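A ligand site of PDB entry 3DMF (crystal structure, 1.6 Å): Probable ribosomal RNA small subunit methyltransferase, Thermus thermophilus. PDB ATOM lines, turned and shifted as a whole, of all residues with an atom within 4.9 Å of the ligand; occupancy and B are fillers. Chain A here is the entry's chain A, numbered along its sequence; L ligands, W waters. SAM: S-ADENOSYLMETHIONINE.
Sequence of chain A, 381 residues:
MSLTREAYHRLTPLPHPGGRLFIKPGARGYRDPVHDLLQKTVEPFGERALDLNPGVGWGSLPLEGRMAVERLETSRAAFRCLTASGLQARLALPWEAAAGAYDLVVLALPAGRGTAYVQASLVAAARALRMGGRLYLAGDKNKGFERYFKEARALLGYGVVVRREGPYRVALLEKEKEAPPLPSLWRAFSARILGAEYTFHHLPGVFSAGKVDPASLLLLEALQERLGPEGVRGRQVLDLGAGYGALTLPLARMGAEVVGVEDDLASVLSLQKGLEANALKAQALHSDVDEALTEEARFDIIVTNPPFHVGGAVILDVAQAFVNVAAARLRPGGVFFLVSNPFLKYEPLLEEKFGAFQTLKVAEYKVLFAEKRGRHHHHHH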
ATOM      1  N   TYR A   8       8.950 -36.685 -15.106  1.00  0.00           N
ATOM      2  CA  TYR A   8       8.953 -35.738 -13.993  1.00  0.00           C
ATOM      3  C   TYR A   8       7.503 -35.302 -13.660  1.00  0.00           C
ATOM      4  O   TYR A   8       7.095 -35.230 -12.485  1.00  0.00           O
ATOM      5  CB  TYR A   8       9.857 -34.502 -14.237  1.00  0.00           C
ATOM      6  CG  TYR A   8       9.679 -33.564 -13.080  1.00  0.00           C
ATOM      7  CD1 TYR A   8      10.310 -33.810 -11.852  1.00  0.00           C
ATOM      8  CD2 TYR A   8       8.727 -32.542 -13.134  1.00  0.00           C
ATOM      9  CE1 TYR A   8      10.061 -33.024 -10.733  1.00  0.00           C
ATOM     10  CE2 TYR A   8       8.454 -31.750 -12.014  1.00  0.00           C
ATOM     11  CZ  TYR A   8       9.120 -31.984 -10.824  1.00  0.00           C
ATOM     12  OH  TYR A   8       8.838 -31.245  -9.703  1.00  0.00           O
ATOM     13  N   PHE A 207      13.395 -19.606   0.630  1.00  0.00           N
ATOM     14  CA  PHE A 207      14.834 -19.781   0.549  1.00  0.00           C
ATOM     15  C   PHE A 207      15.533 -18.458   0.823  1.00  0.00           C
ATOM     16  O   PHE A 207      15.137 -17.411   0.284  1.00  0.00           O
ATOM     17  CB  PHE A 207      15.226 -20.267  -0.849  1.00  0.00           C
ATOM     18  CG  PHE A 207      16.710 -20.302  -1.069  1.00  0.00           C
ATOM     19  CD1 PHE A 207      17.470 -21.324  -0.519  1.00  0.00           C
ATOM     20  CD2 PHE A 207      17.343 -19.329  -1.850  1.00  0.00           C
ATOM     21  CE1 PHE A 207      18.857 -21.377  -0.737  1.00  0.00           C
ATOM     22  CE2 PHE A 207      18.731 -19.363  -2.056  1.00  0.00           C
ATOM     23  CZ  PHE A 207      19.472 -20.412  -1.487  1.00  0.00           C
ATOM     24  N   ASP A 213      21.039 -14.465  -1.453  1.00  0.00           N
ATOM     25  CA  ASP A 213      21.957 -15.594  -1.410  1.00  0.00           C
ATOM     26  C   ASP A 213      23.226 -15.302  -2.213  1.00  0.00           C
ATOM     27  O   ASP A 213      23.142 -14.844  -3.355  1.00  0.00           O
ATOM     28  CB  ASP A 213      21.305 -16.873  -1.939  1.00  0.00           C
ATOM     29  CG  ASP A 213      22.195 -18.078  -1.685  1.00  0.00           C
ATOM     30  OD1 ASP A 213      22.349 -18.496  -0.519  1.00  0.00           O
ATOM     31  OD2 ASP A 213      22.784 -18.575  -2.657  1.00  0.00           O
ATOM     32  N   SER A 216      23.156 -16.655  -5.777  1.00  0.00           N
ATOM     33  CA  SER A 216      22.317 -15.878  -6.667  1.00  0.00           C
ATOM     34  C   SER A 216      23.009 -14.614  -7.173  1.00  0.00           C
ATOM     35  O   SER A 216      22.952 -14.277  -8.369  1.00  0.00           O
ATOM     36  CB  SER A 216      21.001 -15.549  -5.969  1.00  0.00           C
ATOM     37  OG  SER A 216      20.403 -16.750  -5.495  1.00  0.00           O
ATOM     38  N   ASP A 239      12.887 -17.777 -15.115  1.00  0.00           N
ATOM     39  CA  ASP A 239      13.613 -17.951 -13.840  1.00  0.00           C
ATOM     40  C   ASP A 239      13.008 -19.188 -13.186  1.00  0.00           C
ATOM     41  O   ASP A 239      11.856 -19.155 -12.728  1.00  0.00           O
ATOM     42  CB  ASP A 239      13.438 -16.697 -12.961  1.00  0.00           C
ATOM     43  CG  ASP A 239      14.143 -16.792 -11.617  1.00  0.00           C
ATOM     44  OD1 ASP A 239      14.721 -17.835 -11.313  1.00  0.00           O
ATOM     45  OD2 ASP A 239      14.101 -15.773 -10.869  1.00  0.00           O
ATOM     46  N   GLY A 241      12.400 -21.616 -10.419  1.00  0.00           N
ATOM     47  CA  GLY A 241      12.483 -21.605  -8.964  1.00  0.00           C
ATOM     48  C   GLY A 241      12.762 -20.193  -8.479  1.00  0.00           C
ATOM     49  O   GLY A 241      13.792 -19.934  -7.859  1.00  0.00           O
ATOM     50  N   ALA A 242      11.825 -19.280  -8.768  1.00  0.00           N
ATOM     51  CA  ALA A 242      12.090 -17.822  -8.643  1.00  0.00           C
ATOM     52  C   ALA A 242      12.185 -17.325  -7.194  1.00  0.00           C
ATOM     53  O   ALA A 242      12.755 -16.259  -6.947  1.00  0.00           O
ATOM     54  CB  ALA A 242      11.028 -17.010  -9.410  1.00  0.00           C
ATOM     55  N   GLY A 243      11.658 -18.097  -6.233  1.00  0.00           N
ATOM     56  CA  GLY A 243      11.678 -17.627  -4.838  1.00  0.00           C
ATOM     57  C   GLY A 243      11.038 -16.249  -4.672  1.00  0.00           C
ATOM     58  O   GLY A 243      10.051 -15.938  -5.354  1.00  0.00           O
ATOM     59  N   ALA A 246      15.205 -12.926  -6.106  1.00  0.00           N
ATOM     60  CA  ALA A 246      16.602 -12.434  -6.092  1.00  0.00           C
ATOM     61  C   ALA A 246      17.152 -12.333  -7.519  1.00  0.00           C
ATOM     62  O   ALA A 246      17.932 -11.430  -7.817  1.00  0.00           O
ATOM     63  CB  ALA A 246      17.481 -13.305  -5.215  1.00  0.00           C
ATOM     64  N   LEU A 247      16.748 -13.250  -8.410  1.00  0.00           N
ATOM     65  CA  LEU A 247      17.164 -13.116  -9.814  1.00  0.00           C
ATOM     66  C   LEU A 247      16.108 -12.330 -10.608  1.00  0.00           C
ATOM     67  O   LEU A 247      16.448 -11.540 -11.499  1.00  0.00           O
ATOM     68  CB  LEU A 247      17.377 -14.486 -10.461  1.00  0.00           C
ATOM     69  CG  LEU A 247      18.346 -15.431  -9.744  1.00  0.00           C
ATOM     70  CD1 LEU A 247      18.442 -16.770 -10.476  1.00  0.00           C
ATOM     71  CD2 LEU A 247      19.728 -14.794  -9.615  1.00  0.00           C
ATOM     72  N   VAL A 261       8.831 -19.045 -12.359  1.00  0.00           N
ATOM     73  CA  VAL A 261       8.005 -20.209 -11.938  1.00  0.00           C
ATOM     74  C   VAL A 261       8.504 -20.672 -10.575  1.00  0.00           C
ATOM     75  O   VAL A 261       9.716 -20.769 -10.329  1.00  0.00           O
ATOM     76  CB  VAL A 261       7.994 -21.376 -12.945  1.00  0.00           C
ATOM     77  CG1 VAL A 261       7.245 -20.971 -14.220  1.00  0.00           C
ATOM     78  CG2 VAL A 261       9.422 -21.886 -13.293  1.00  0.00           C
ATOM     79  N   GLU A 262       7.550 -20.937  -9.693  1.00  0.00           N
ATOM     80  CA  GLU A 262       7.881 -21.280  -8.310  1.00  0.00           C
ATOM     81  C   GLU A 262       6.808 -22.203  -7.734  1.00  0.00           C
ATOM     82  O   GLU A 262       5.604 -21.918  -7.841  1.00  0.00           O
ATOM     83  CB  GLU A 262       7.984 -19.962  -7.531  1.00  0.00           C
ATOM     84  CG  GLU A 262       8.016 -20.103  -6.002  1.00  0.00           C
ATOM     85  CD  GLU A 262       9.198 -20.914  -5.528  1.00  0.00           C
ATOM     86  OE1 GLU A 262      10.364 -20.560  -5.875  1.00  0.00           O
ATOM     87  OE2 GLU A 262       8.974 -21.925  -4.816  1.00  0.00           O
ATOM     88  N   ASP A 263       7.239 -23.320  -7.160  1.00  0.00           N
ATOM     89  CA  ASP A 263       6.306 -24.329  -6.668  1.00  0.00           C
ATOM     90  C   ASP A 263       5.633 -23.966  -5.349  1.00  0.00           C
ATOM     91  O   ASP A 263       4.547 -24.482  -5.060  1.00  0.00           O
ATOM     92  CB  ASP A 263       7.019 -25.674  -6.523  1.00  0.00           C
ATOM     93  CG  ASP A 263       6.065 -26.799  -6.182  1.00  0.00           C
ATOM     94  OD1 ASP A 263       5.191 -27.112  -7.026  1.00  0.00           O
ATOM     95  OD2 ASP A 263       6.222 -27.422  -5.093  1.00  0.00           O
ATOM     96  N   ASP A 264       6.277 -23.104  -4.556  1.00  0.00           N
ATOM     97  CA  ASP A 264       5.813 -22.769  -3.196  1.00  0.00           C
ATOM     98  C   ASP A 264       4.957 -21.478  -3.217  1.00  0.00           C
ATOM     99  O   ASP A 264       5.462 -20.387  -3.539  1.00  0.00           O
ATOM    100  CB  ASP A 264       7.013 -22.586  -2.239  1.00  0.00           C
ATOM    101  CG  ASP A 264       6.613 -21.948  -0.919  1.00  0.00           C
ATOM    102  OD1 ASP A 264       5.597 -22.355  -0.359  1.00  0.00           O
ATOM    103  OD2 ASP A 264       7.344 -21.049  -0.424  1.00  0.00           O
ATOM    104  N   SER A 267       6.356 -18.381  -1.467  1.00  0.00           N
ATOM    105  CA  SER A 267       7.379 -17.750  -2.300  1.00  0.00           C
ATOM    106  C   SER A 267       6.787 -16.951  -3.467  1.00  0.00           C
ATOM    107  O   SER A 267       7.250 -15.833  -3.745  1.00  0.00           O
ATOM    108  CB  SER A 267       8.392 -18.792  -2.769  1.00  0.00           C
ATOM    109  OG  SER A 267       9.093 -19.289  -1.642  1.00  0.00           O
ATOM    110  N   SER A 287       3.807 -22.701  -9.948  1.00  0.00           N
ATOM    111  CA  SER A 287       4.007 -23.723 -10.985  1.00  0.00           C
ATOM    112  C   SER A 287       4.976 -24.788 -10.518  1.00  0.00           C
ATOM    113  O   SER A 287       5.960 -24.479  -9.874  1.00  0.00           O
ATOM    114  CB  SER A 287       4.589 -23.045 -12.235  1.00  0.00           C
ATOM    115  OG  SER A 287       4.728 -23.946 -13.337  1.00  0.00           O
ATOM    116  N   ASP A 288       4.669 -26.042 -10.837  1.00  0.00           N
ATOM    117  CA  ASP A 288       5.611 -27.150 -10.615  1.00  0.00           C
ATOM    118  C   ASP A 288       6.498 -27.176 -11.858  1.00  0.00           C
ATOM    119  O   ASP A 288       6.080 -27.620 -12.932  1.00  0.00           O
ATOM    120  CB  ASP A 288       4.851 -28.464 -10.513  1.00  0.00           C
ATOM    121  CG  ASP A 288       5.765 -29.665 -10.326  1.00  0.00           C
ATOM    122  OD1 ASP A 288       6.970 -29.455 -10.007  1.00  0.00           O
ATOM    123  OD2 ASP A 288       5.247 -30.780 -10.445  1.00  0.00           O
ATOM    124  N   VAL A 289       7.710 -26.657 -11.695  1.00  0.00           N
ATOM    125  CA  VAL A 289       8.639 -26.404 -12.822  1.00  0.00           C
ATOM    126  C   VAL A 289       7.872 -25.598 -13.902  1.00  0.00           C
ATOM    127  O   VAL A 289       7.342 -24.517 -13.592  1.00  0.00           O
ATOM    128  CB  VAL A 289       9.348 -27.693 -13.319  1.00  0.00           C
ATOM    129  CG1 VAL A 289      10.572 -27.320 -14.174  1.00  0.00           C
ATOM    130  CG2 VAL A 289       9.810 -28.561 -12.125  1.00  0.00           C
ATOM    131  N   ASN A 305      18.933 -20.749  -9.750  1.00  0.00           N
ATOM    132  CA  ASN A 305      19.614 -21.269  -8.559  1.00  0.00           C
ATOM    133  C   ASN A 305      18.727 -22.432  -8.074  1.00  0.00           C
ATOM    134  O   ASN A 305      17.733 -22.198  -7.372  1.00  0.00           O
ATOM    135  CB  ASN A 305      19.760 -20.176  -7.499  1.00  0.00           C
ATOM    136  CG  ASN A 305      20.497 -20.656  -6.288  1.00  0.00           C
ATOM    137  OD1 ASN A 305      20.784 -21.850  -6.172  1.00  0.00           O
ATOM    138  ND2 ASN A 305      20.830 -19.746  -5.362  1.00  0.00           N
ATOM    139  N   PRO A 306      19.021 -23.675  -8.488  1.00  0.00           N
ATOM    140  CA  PRO A 306      18.111 -24.787  -8.190  1.00  0.00           C
ATOM    141  C   PRO A 306      18.121 -25.199  -6.730  1.00  0.00           C
ATOM    142  O   PRO A 306      19.101 -24.921  -6.017  1.00  0.00           O
ATOM    143  CB  PRO A 306      18.638 -25.954  -9.072  1.00  0.00           C
ATOM    144  CG  PRO A 306      19.626 -25.374  -9.957  1.00  0.00           C
ATOM    145  CD  PRO A 306      20.171 -24.124  -9.287  1.00  0.00           C
ATOM    146  N   PRO A 307      17.067 -25.887  -6.275  1.00  0.00           N
ATOM    147  CA  PRO A 307      17.064 -26.391  -4.913  1.00  0.00           C
ATOM    148  C   PRO A 307      18.156 -27.446  -4.729  1.00  0.00           C
ATOM    149  O   PRO A 307      18.617 -28.057  -5.720  1.00  0.00           O
ATOM    150  CB  PRO A 307      15.682 -27.033  -4.785  1.00  0.00           C
ATOM    151  CG  PRO A 307      15.262 -27.354  -6.155  1.00  0.00           C
ATOM    152  CD  PRO A 307      15.873 -26.301  -7.033  1.00  0.00           C
ATOM    153  N   PHE A 308      18.584 -27.629  -3.487  1.00  0.00           N
ATOM    154  CA  PHE A 308      19.609 -28.634  -3.156  1.00  0.00           C
ATOM    155  C   PHE A 308      19.367 -29.176  -1.767  1.00  0.00           C
ATOM    156  O   PHE A 308      18.770 -28.497  -0.929  1.00  0.00           O
ATOM    157  CB  PHE A 308      21.023 -28.072  -3.259  1.00  0.00           C
ATOM    158  CG  PHE A 308      21.244 -26.808  -2.451  1.00  0.00           C
ATOM    159  CD1 PHE A 308      21.773 -26.874  -1.175  1.00  0.00           C
ATOM    160  CD2 PHE A 308      20.911 -25.554  -2.988  1.00  0.00           C
ATOM    161  CE1 PHE A 308      21.981 -25.707  -0.421  1.00  0.00           C
ATOM    162  CE2 PHE A 308      21.106 -24.390  -2.239  1.00  0.00           C
ATOM    163  CZ  PHE A 308      21.642 -24.476  -0.956  1.00  0.00           C
ATOM    164  N   VAL A 318      13.902 -32.432  -8.828  1.00  0.00           N
ATOM    165  CA  VAL A 318      13.440 -31.126  -9.322  1.00  0.00           C
ATOM    166  C   VAL A 318      14.555 -30.390 -10.050  1.00  0.00           C
ATOM    167  O   VAL A 318      14.341 -29.832 -11.125  1.00  0.00           O
ATOM    168  CB  VAL A 318      12.854 -30.220  -8.178  1.00  0.00           C
ATOM    169  CG1 VAL A 318      12.660 -28.788  -8.641  1.00  0.00           C
ATOM    170  CG2 VAL A 318      11.530 -30.802  -7.663  1.00  0.00           C
ATOM    171  N   PHE A 322      14.849 -29.134 -13.820  1.00  0.00           N
ATOM    172  CA  PHE A 322      15.163 -27.759 -14.225  1.00  0.00           C
ATOM    173  C   PHE A 322      16.072 -27.730 -15.464  1.00  0.00           C
ATOM    174  O   PHE A 322      15.842 -26.965 -16.421  1.00  0.00           O
ATOM    175  CB  PHE A 322      15.865 -26.983 -13.097  1.00  0.00           C
ATOM    176  CG  PHE A 322      14.923 -26.406 -12.059  1.00  0.00           C
ATOM    177  CD1 PHE A 322      13.573 -26.791 -11.969  1.00  0.00           C
ATOM    178  CD2 PHE A 322      15.405 -25.465 -11.161  1.00  0.00           C
ATOM    179  CE1 PHE A 322      12.757 -26.224 -10.983  1.00  0.00           C
ATOM    180  CE2 PHE A 322      14.598 -24.893 -10.201  1.00  0.00           C
ATOM    181  CZ  PHE A 322      13.262 -25.286 -10.107  1.00  0.00           C
HETATM  182  N   SAM L   1      15.727 -17.929  -7.383  1.00  0.00           N
HETATM  183  CA  SAM L   1      15.671 -17.679  -5.905  1.00  0.00           C
HETATM  184  C   SAM L   1      16.998 -17.109  -5.429  1.00  0.00           C
HETATM  185  O   SAM L   1      17.969 -17.208  -6.180  1.00  0.00           O
HETATM  186  OXT SAM L   1      17.085 -16.598  -4.321  1.00  0.00           O
HETATM  187  CB  SAM L   1      15.375 -18.932  -5.091  1.00  0.00           C
HETATM  188  CG  SAM L   1      16.387 -20.074  -5.284  1.00  0.00           C
HETATM  189  SD  SAM L   1      16.106 -21.495  -4.195  1.00  0.00           S
HETATM  190  CE  SAM L   1      17.756 -22.252  -4.162  1.00  0.00           C
HETATM  191  C5' SAM L   1      15.266 -22.694  -5.264  1.00  0.00           C
HETATM  192  C4' SAM L   1      13.767 -22.381  -5.448  1.00  0.00           C
HETATM  193  O4' SAM L   1      13.234 -23.487  -6.184  1.00  0.00           O
HETATM  194  C3' SAM L   1      12.962 -22.214  -4.151  1.00  0.00           C
HETATM  195  O3' SAM L   1      12.298 -20.981  -4.158  1.00  0.00           O
HETATM  196  C2' SAM L   1      12.007 -23.406  -4.225  1.00  0.00           C
HETATM  197  O2' SAM L   1      10.764 -23.259  -3.517  1.00  0.00           O
HETATM  198  C1' SAM L   1      11.899 -23.600  -5.732  1.00  0.00           C
HETATM  199  N9  SAM L   1      11.354 -24.911  -6.103  1.00  0.00           N
HETATM  200  C8  SAM L   1      11.458 -26.120  -5.451  1.00  0.00           C
HETATM  201  N7  SAM L   1      10.796 -27.066  -6.183  1.00  0.00           N
HETATM  202  C5  SAM L   1      10.255 -26.453  -7.272  1.00  0.00           C
HETATM  203  C6  SAM L   1       9.465 -26.907  -8.320  1.00  0.00           C
HETATM  204  N6  SAM L   1       9.023 -28.164  -8.427  1.00  0.00           N
HETATM  205  N1  SAM L   1       9.103 -25.991  -9.283  1.00  0.00           N
HETATM  206  C2  SAM L   1       9.458 -24.670  -9.230  1.00  0.00           C
HETATM  207  N3  SAM L   1      10.210 -24.184  -8.173  1.00  0.00           N
HETATM  208  C4  SAM L   1      10.609 -25.101  -7.229  1.00  0.00           C
HETATM  209  O   HOH W   1      14.850 -15.444  -8.434  1.00  0.00           O
HETATM  210  O   HOH W   2      14.837 -14.991  -4.021  1.00  0.00           O
HETATM  211  O   HOH W   3       8.405 -29.301  -5.742  1.00  0.00           O
HETATM  212  O   HOH W   4      16.206 -19.569  -9.602  1.00  0.00           O
HETATM  213  O   HOH W   5      18.400 -14.935  -2.405  1.00  0.00           O
HETATM  214  O   HOH W   6      11.854 -19.519  -1.864  1.00  0.00           O
HETATM  215  O   HOH W   7       9.521 -25.488  -2.247  1.00  0.00           O
HETATM  216  O   HOH W   8      15.241 -24.203  -2.129  1.00  0.00           O
HETATM  217  O   HOH W   9      10.680 -29.286  -4.129  1.00  0.00           O
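The side-chain hydroxyl of Ser 216 sits at hydrogen-bond distance from an oxygen (O) of the ligand (2.6 Å). OE2 of Glu 262 lies within hydrogen-bond range of O2' of the ligand (2.6 Å). A nitrogen (N) of the ligand sits at hydrogen-bond distance from the backbone carbonyl oxygen (O) of Gly 241 (2.8 Å). N1 of the ligand lies within hydrogen-bond range of N of Val 289 (2.9 Å). The side-chain carboxylate of Asp 288 lies within hydrogen-bond range of a nitrogen (N6) of the ligand, at 2.9 Å. A nitrogen (N3) of the ligand sits at hydrogen-bond distance from the backbone NH (N) of Asp 263, 3.3 Å away. OH of Tyr 8 sits at hydrogen-bond distance from N6 of the ligand (3.3 Å). N of the ligand lies close to O of Ala 242 (3.4 Å).
OG of Ser 216 lies within hydrogen-bond range of ND2 of Asn 305, at 3.0 Å. The backbone NH (N) of Ala 242 sits at hydrogen-bond distance from the side-chain carboxylate (OE1) of Glu 262, 3.5 Å away. The backbone carbonyl oxygen of Glu 262 sits at hydrogen-bond distance from the backbone NH of Ser 287 (2.9 Å). The backbone NH (N) of Asp 264 sits at hydrogen-bond distance from the side-chain carboxylate (OE2) of Glu 262, at 3.0 Å. The backbone carbonyl oxygen (O) of Val 261 is in hydrogen-bond range of the backbone NH (N) of Gly 241. O of Val 289 sits at hydrogen-bond distance from OG of Ser 287 (2.7 Å). O of Ser 287 sits at hydrogen-bond distance from N of Asp 263. The backbone NH of Ala 242 lies within hydrogen-bond range of the backbone carbonyl oxygen of Val 261, 3.0 Å away.
SD of the ligand lies close to O of Asn 305, 3.6 Å away. Residues that only touch the ligand: Phe 207, Gly 243, Ala 246, Ser 287, Pro 306, Pro 307, Val 318 and Phe 322. The nearest printed residue that does not touch the ligand is Leu 247 (4.0002 Å).
Water W6 lies within hydrogen-bond range of O3' of the ligand, OG of Ser 267 and N of Phe 207. Water W2 lies within hydrogen-bond range of OXT of the ligand (2.8 Å) and N of Ala 246 (3.0 Å). Water W4 lies within hydrogen-bond range of N of the ligand, OD1 of Asp 239, N of Asn 305 and O of Gly 241. Water W1 lies within hydrogen-bond range of OD2 of Asp 239 (2.6 Å), O of Ala 242 (2.7 Å), N of the ligand (2.8 Å), N of Leu 247 (2.9 Å) and N of Ala 246 (3.4 Å). Water W5 lies within hydrogen-bond range of N of Asp 213 and OXT of the ligand. Water W3 bridges OD2 of Asp 263 and N6 of the ligand.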
